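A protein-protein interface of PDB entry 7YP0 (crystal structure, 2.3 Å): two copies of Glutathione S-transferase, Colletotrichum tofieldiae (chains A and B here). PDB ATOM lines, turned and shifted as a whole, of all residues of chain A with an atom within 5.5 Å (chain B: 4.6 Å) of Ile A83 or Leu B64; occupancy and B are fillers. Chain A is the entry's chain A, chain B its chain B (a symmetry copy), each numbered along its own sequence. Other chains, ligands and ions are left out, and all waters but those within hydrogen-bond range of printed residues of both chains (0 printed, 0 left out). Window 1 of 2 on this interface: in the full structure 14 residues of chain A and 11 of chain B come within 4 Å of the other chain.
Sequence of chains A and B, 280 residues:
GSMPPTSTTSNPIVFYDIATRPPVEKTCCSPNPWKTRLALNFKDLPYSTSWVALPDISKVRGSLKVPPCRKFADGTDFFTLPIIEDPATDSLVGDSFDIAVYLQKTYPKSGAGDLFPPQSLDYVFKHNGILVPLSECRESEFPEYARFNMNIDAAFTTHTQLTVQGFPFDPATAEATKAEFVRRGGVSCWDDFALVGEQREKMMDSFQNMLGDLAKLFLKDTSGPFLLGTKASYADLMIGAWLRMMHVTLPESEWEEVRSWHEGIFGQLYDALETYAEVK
2 positions are printed for both chains.
N of Ser B63 lies within hydrogen-bond range of O of Gly A94.
Of the printed residues of chain B, Ile A83 touches Leu B64 (3.9 Å).
Leu B64 touches just these residues of chain A: Ile A83, Leu A92 and Gly A94.
Of the printed residues of chain B, Asp A95 touches Ser B63.
Of the printed residues of chain B, Gly A94 touches Gly B62, Ser B63 and Leu B64.
Printed residues of chain A within 4 Å of Gly B62: Gly A94 (3.5 Å).
Printed residues of chain B within 4 Å of Leu A92: Leu B64 (3.8 Å).
Ile A84 touches none of the printed residues of chain B.
The backbone carbonyl oxygen (O) of Ile A83 is in hydrogen-bond range of the backbone NH (N) of Tyr A16, at 2.8 Å.
The backbone carbonyl oxygen of Pro A82 lies within hydrogen-bond range of the backbone NH of Asp A95 (3.0 Å).
Among the printed residues, pairs that only touch across the chains: Gly A94 with Gly B62 (3.5 Å), Asp A95 with Ser B63 (3.7 Å), Gly A94 with Leu B64 (3.8 Å), Leu A92 with Leu B64 (3.8 Å) and Ile A83 with Leu B64 (3.9 Å).
Printed residues of chain A that touch a printed residue of chain B: Ile A83, Leu A92, Gly A94 and Asp A95.
Hydrophobic or aromatic side chains of chain A that line the printed part of chain B: Ile A83 and Leu A92.
Printed residues of chain B that touch a printed residue of chain A: Gly B62, Ser B63 and Leu B64.
Hydrophobic or aromatic side chains of chain B that line the printed part of chain A: Leu B64.
Among the printed residues, 6 pairs touch across the chains.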
ATOM      1  N   VAL A  14       8.868  26.595   6.622  1.00  0.00           N
ATOM      2  CA  VAL A  14       7.770  26.348   7.556  1.00  0.00           C
ATOM      3  C   VAL A  14       8.385  25.944   8.886  1.00  0.00           C
ATOM      4  O   VAL A  14       9.213  25.026   8.941  1.00  0.00           O
ATOM      5  CB  VAL A  14       6.793  25.273   7.042  1.00  0.00           C
ATOM      6  CG1 VAL A  14       5.778  24.927   8.120  1.00  0.00           C
ATOM      7  CG2 VAL A  14       6.064  25.775   5.799  1.00  0.00           C
ATOM      8  N   PHE A  15       7.985  26.635   9.952  1.00  0.00           N
ATOM      9  CA  PHE A  15       8.600  26.517  11.269  1.00  0.00           C
ATOM     10  C   PHE A  15       7.519  26.030  12.221  1.00  0.00           C
ATOM     11  O   PHE A  15       6.448  26.631  12.286  1.00  0.00           O
ATOM     12  CB  PHE A  15       9.196  27.877  11.683  1.00  0.00           C
ATOM     13  CG  PHE A  15       9.636  27.969  13.114  1.00  0.00           C
ATOM     14  CD1 PHE A  15      10.416  26.989  13.694  1.00  0.00           C
ATOM     15  CD2 PHE A  15       9.286  29.065  13.879  1.00  0.00           C
ATOM     16  CE1 PHE A  15      10.807  27.077  15.032  1.00  0.00           C
ATOM     17  CE2 PHE A  15       9.675  29.171  15.202  1.00  0.00           C
ATOM     18  CZ  PHE A  15      10.437  28.174  15.781  1.00  0.00           C
ATOM     19  N   TYR A  16       7.772  24.912  12.911  1.00  0.00           N
ATOM     20  CA  TYR A  16       6.791  24.299  13.810  1.00  0.00           C
ATOM     21  C   TYR A  16       7.122  24.631  15.263  1.00  0.00           C
ATOM     22  O   TYR A  16       8.180  24.247  15.768  1.00  0.00           O
ATOM     23  CB  TYR A  16       6.722  22.785  13.612  1.00  0.00           C
ATOM     24  CG  TYR A  16       6.028  22.439  12.334  1.00  0.00           C
ATOM     25  CD1 TYR A  16       4.647  22.413  12.258  1.00  0.00           C
ATOM     26  CD2 TYR A  16       6.756  22.196  11.184  1.00  0.00           C
ATOM     27  CE1 TYR A  16       4.009  22.133  11.067  1.00  0.00           C
ATOM     28  CE2 TYR A  16       6.139  21.917   9.998  1.00  0.00           C
ATOM     29  CZ  TYR A  16       4.768  21.888   9.934  1.00  0.00           C
ATOM     30  OH  TYR A  16       4.157  21.612   8.727  1.00  0.00           O
ATOM     31  N   THR A  80       9.768  17.201  20.989  1.00  0.00           N
ATOM     32  CA  THR A  80      10.053  16.897  19.596  1.00  0.00           C
ATOM     33  C   THR A  80      10.036  18.138  18.703  1.00  0.00           C
ATOM     34  O   THR A  80      10.260  18.008  17.496  1.00  0.00           O
ATOM     35  CB  THR A  80       9.039  15.840  19.100  1.00  0.00           C
ATOM     36  OG1 THR A  80       9.118  15.702  17.680  1.00  0.00           O
ATOM     37  CG2 THR A  80       7.610  16.187  19.470  1.00  0.00           C
ATOM     38  N   LEU A  81       9.848  19.347  19.251  1.00  0.00           N
ATOM     39  CA  LEU A  81       9.040  20.228  18.420  1.00  0.00           C
ATOM     40  C   LEU A  81       9.670  21.361  17.632  1.00  0.00           C
ATOM     41  O   LEU A  81       9.015  21.841  16.697  1.00  0.00           O
ATOM     42  CB  LEU A  81       7.914  20.851  19.222  1.00  0.00           C
ATOM     43  CG  LEU A  81       6.620  20.674  18.417  1.00  0.00           C
ATOM     44  CD1 LEU A  81       6.013  22.006  18.132  1.00  0.00           C
ATOM     45  CD2 LEU A  81       6.829  19.914  17.105  1.00  0.00           C
ATOM     46  N   PRO A  82      10.852  21.841  17.900  1.00  0.00           N
ATOM     47  CA  PRO A  82      11.423  22.691  16.853  1.00  0.00           C
ATOM     48  C   PRO A  82      11.629  21.796  15.626  1.00  0.00           C
ATOM     49  O   PRO A  82      12.506  20.932  15.633  1.00  0.00           O
ATOM     50  CB  PRO A  82      12.721  23.242  17.462  1.00  0.00           C
ATOM     51  CG  PRO A  82      12.678  22.892  18.892  1.00  0.00           C
ATOM     52  CD  PRO A  82      11.611  21.858  19.158  1.00  0.00           C
ATOM     53  N   ILE A  83      10.769  21.927  14.608  1.00  0.00           N
ATOM     54  CA  ILE A  83      10.964  21.301  13.300  1.00  0.00           C
ATOM     55  C   ILE A  83      10.799  22.376  12.232  1.00  0.00           C
ATOM     56  O   ILE A  83       9.891  23.207  12.323  1.00  0.00           O
ATOM     57  CB  ILE A  83       9.969  20.140  13.043  1.00  0.00           C
ATOM     58  CG1 ILE A  83      10.264  18.948  13.941  1.00  0.00           C
ATOM     59  CG2 ILE A  83      10.007  19.668  11.578  1.00  0.00           C
ATOM     60  CD1 ILE A  83       9.093  17.995  14.044  1.00  0.00           C
ATOM     61  N   ILE A  84      11.657  22.357  11.208  1.00  0.00           N
ATOM     62  CA  ILE A  84      11.430  23.203  10.040  1.00  0.00           C
ATOM     63  C   ILE A  84      11.382  22.353   8.775  1.00  0.00           C
ATOM     64  O   ILE A  84      12.039  21.314   8.662  1.00  0.00           O
ATOM     65  CB  ILE A  84      12.492  24.318   9.892  1.00  0.00           C
ATOM     66  CG1 ILE A  84      13.892  23.724   9.787  1.00  0.00           C
ATOM     67  CG2 ILE A  84      12.412  25.305  11.039  1.00  0.00           C
ATOM     68  CD1 ILE A  84      14.804  24.508   8.867  1.00  0.00           C
ATOM     69  N   GLU A  85      10.592  22.812   7.815  1.00  0.00           N
ATOM     70  CA  GLU A  85      10.641  22.325   6.445  1.00  0.00           C
ATOM     71  C   GLU A  85      11.203  23.439   5.573  1.00  0.00           C
ATOM     72  O   GLU A  85      10.656  24.548   5.548  1.00  0.00           O
ATOM     73  CB  GLU A  85       9.256  21.891   5.956  1.00  0.00           C
ATOM     74  CG  GLU A  85       9.178  21.463   4.475  1.00  0.00           C
ATOM     75  CD  GLU A  85       8.237  22.335   3.608  1.00  0.00           C
ATOM     76  OE1 GLU A  85       8.716  22.864   2.582  1.00  0.00           O
ATOM     77  OE2 GLU A  85       7.011  22.457   3.912  1.00  0.00           O
ATOM     78  N   LEU A  92      13.537  18.185   5.862  1.00  0.00           N
ATOM     79  CA  LEU A  92      12.768  18.242   7.092  1.00  0.00           C
ATOM     80  C   LEU A  92      13.768  18.024   8.209  1.00  0.00           C
ATOM     81  O   LEU A  92      14.398  16.963   8.264  1.00  0.00           O
ATOM     82  CB  LEU A  92      11.682  17.159   7.100  1.00  0.00           C
ATOM     83  CG  LEU A  92      10.381  17.373   7.857  1.00  0.00           C
ATOM     84  CD1 LEU A  92       9.733  18.677   7.430  1.00  0.00           C
ATOM     85  CD2 LEU A  92       9.442  16.207   7.588  1.00  0.00           C
ATOM     86  N   VAL A  93      13.948  19.030   9.072  1.00  0.00           N
ATOM     87  CA  VAL A  93      15.008  19.026  10.077  1.00  0.00           C
ATOM     88  C   VAL A  93      14.404  19.284  11.452  1.00  0.00           C
ATOM     89  O   VAL A  93      13.716  20.291  11.659  1.00  0.00           O
ATOM     90  CB  VAL A  93      16.098  20.079   9.769  1.00  0.00           C
ATOM     91  CG1 VAL A  93      17.317  19.874  10.678  1.00  0.00           C
ATOM     92  CG2 VAL A  93      16.511  20.019   8.303  1.00  0.00           C
ATOM     93  N   GLY A  94      14.677  18.392  12.391  1.00  0.00           N
ATOM     94  CA  GLY A  94      14.214  18.593  13.748  1.00  0.00           C
ATOM     95  C   GLY A  94      15.358  18.846  14.708  1.00  0.00           C
ATOM     96  O   GLY A  94      16.522  18.587  14.367  1.00  0.00           O
ATOM     97  N   ASP A  95      15.027  19.361  15.900  1.00  0.00           N
ATOM     98  CA  ASP A  95      15.980  19.642  16.970  1.00  0.00           C
ATOM     99  C   ASP A  95      16.701  20.965  16.702  1.00  0.00           C
ATOM    100  O   ASP A  95      17.230  21.186  15.609  1.00  0.00           O
ATOM    101  CB  ASP A  95      16.949  18.464  17.138  1.00  0.00           C
ATOM    102  CG  ASP A  95      18.083  18.761  18.078  1.00  0.00           C
ATOM    103  OD1 ASP A  95      19.077  19.375  17.628  1.00  0.00           O
ATOM    104  OD2 ASP A  95      17.981  18.380  19.269  1.00  0.00           O
ATOM    105  N   ILE A  99      19.037  22.253  13.593  1.00  0.00           N
ATOM    106  CA  ILE A  99      18.471  23.242  12.688  1.00  0.00           C
ATOM    107  C   ILE A  99      19.435  24.410  12.519  1.00  0.00           C
ATOM    108  O   ILE A  99      19.587  24.950  11.419  1.00  0.00           O
ATOM    109  CB  ILE A  99      17.101  23.716  13.197  1.00  0.00           C
ATOM    110  CG1 ILE A  99      16.062  22.603  13.038  1.00  0.00           C
ATOM    111  CG2 ILE A  99      16.673  24.939  12.440  1.00  0.00           C
ATOM    112  CD1 ILE A  99      14.794  22.842  13.833  1.00  0.00           C
ATOM    113  N   PRO B  55      13.803  11.743   5.500  1.00  0.00           N
ATOM    114  CA  PRO B  55      14.760  12.099   6.564  1.00  0.00           C
ATOM    115  C   PRO B  55      15.416  10.889   7.195  1.00  0.00           C
ATOM    116  O   PRO B  55      16.531  11.014   7.722  1.00  0.00           O
ATOM    117  CB  PRO B  55      13.901  12.866   7.584  1.00  0.00           C
ATOM    118  CG  PRO B  55      12.572  13.060   6.937  1.00  0.00           C
ATOM    119  CD  PRO B  55      12.415  12.009   5.899  1.00  0.00           C
ATOM    120  N   ASP B  56      14.753   9.723   7.144  1.00  0.00           N
ATOM    121  CA  ASP B  56      15.311   8.509   7.734  1.00  0.00           C
ATOM    122  C   ASP B  56      16.671   8.163   7.135  1.00  0.00           C
ATOM    123  O   ASP B  56      17.509   7.566   7.814  1.00  0.00           O
ATOM    124  CB  ASP B  56      14.356   7.320   7.547  1.00  0.00           C
ATOM    125  CG  ASP B  56      12.892   7.654   7.864  1.00  0.00           C
ATOM    126  OD1 ASP B  56      12.266   6.880   8.625  1.00  0.00           O
ATOM    127  OD2 ASP B  56      12.344   8.650   7.321  1.00  0.00           O
ATOM    128  N   GLY B  62      19.678  15.440  12.555  1.00  0.00           N
ATOM    129  CA  GLY B  62      18.402  15.931  13.058  1.00  0.00           C
ATOM    130  C   GLY B  62      17.767  14.909  13.987  1.00  0.00           C
ATOM    131  O   GLY B  62      18.336  13.844  14.266  1.00  0.00           O
ATOM    132  N   SER B  63      16.560  15.241  14.455  1.00  0.00           N
ATOM    133  CA  SER B  63      15.818  14.386  15.377  1.00  0.00           C
ATOM    134  C   SER B  63      14.700  13.581  14.706  1.00  0.00           C
ATOM    135  O   SER B  63      13.995  12.840  15.403  1.00  0.00           O
ATOM    136  CB  SER B  63      15.230  15.227  16.518  1.00  0.00           C
ATOM    137  N   LEU B  64      14.525  13.696  13.382  1.00  0.00           N
ATOM    138  CA  LEU B  64      13.462  12.992  12.648  1.00  0.00           C
ATOM    139  C   LEU B  64      14.066  11.814  11.883  1.00  0.00           C
ATOM    140  O   LEU B  64      14.239  11.849  10.665  1.00  0.00           O
ATOM    141  CB  LEU B  64      12.748  13.940  11.688  1.00  0.00           C
ATOM    142  CG  LEU B  64      11.796  15.016  12.200  1.00  0.00           C
ATOM    143  CD1 LEU B  64      11.810  16.175  11.217  1.00  0.00           C
ATOM    144  CD2 LEU B  64      10.383  14.476  12.365  1.00  0.00           C
ATOM    145  N   LYS B  65      14.377  10.744  12.613  1.00  0.00           N
ATOM    146  CA  LYS B  65      15.030   9.585  12.018  1.00  0.00           C
ATOM    147  C   LYS B  65      14.249   8.285  12.169  1.00  0.00           C
ATOM    148  O   LYS B  65      14.559   7.320  11.462  1.00  0.00           O
ATOM    149  CB  LYS B  65      16.433   9.380  12.623  1.00  0.00           C
ATOM    150  CG  LYS B  65      17.347  10.612  12.633  1.00  0.00           C
ATOM    151  CD  LYS B  65      17.594  11.199  11.236  1.00  0.00           C
ATOM    152  CE  LYS B  65      18.326  10.232  10.295  1.00  0.00           C
ATOM    153  NZ  LYS B  65      19.213   9.253  10.990  1.00  0.00           N
ATOM    154  N   VAL B  66      13.262   8.226  13.057  1.00  0.00           N
ATOM    155  CA  VAL B  66      12.504   6.996  13.271  1.00  0.00           C
ATOM    156  C   VAL B  66      11.011   7.285  13.170  1.00  0.00           C
ATOM    157  O   VAL B  66      10.563   8.382  13.545  1.00  0.00           O
ATOM    158  CB  VAL B  66      12.836   6.367  14.631  1.00  0.00           C
ATOM    159  CG1 VAL B  66      14.234   5.743  14.599  1.00  0.00           C
ATOM    160  CG2 VAL B  66      12.687   7.406  15.743  1.00  0.00           C
ATOM    161  N   THR B  80       9.430   7.683   8.697  1.00  0.00           N
ATOM    162  CA  THR B  80       8.852   8.830   9.370  1.00  0.00           C
ATOM    163  C   THR B  80       7.738   9.478   8.553  1.00  0.00           C
ATOM    164  O   THR B  80       6.898  10.165   9.131  1.00  0.00           O
ATOM    165  CB  THR B  80       9.933   9.881   9.688  1.00  0.00           C
ATOM    166  OG1 THR B  80      10.438  10.450   8.477  1.00  0.00           O
ATOM    167  CG2 THR B  80      11.100   9.284  10.467  1.00  0.00           C
ATOM    168  N   LEU B  92      -0.314  17.859  14.584  1.00  0.00           N
ATOM    169  CA  LEU B  92       0.772  17.311  13.779  1.00  0.00           C
ATOM    170  C   LEU B  92       0.766  15.814  14.046  1.00  0.00           C
ATOM    171  O   LEU B  92       0.993  15.398  15.183  1.00  0.00           O
ATOM    172  CB  LEU B  92       2.107  17.944  14.158  1.00  0.00           C
ATOM    173  CG  LEU B  92       3.314  17.593  13.301  1.00  0.00           C
ATOM    174  CD1 LEU B  92       3.109  18.132  11.894  1.00  0.00           C
ATOM    175  CD2 LEU B  92       4.592  18.147  13.948  1.00  0.00           C
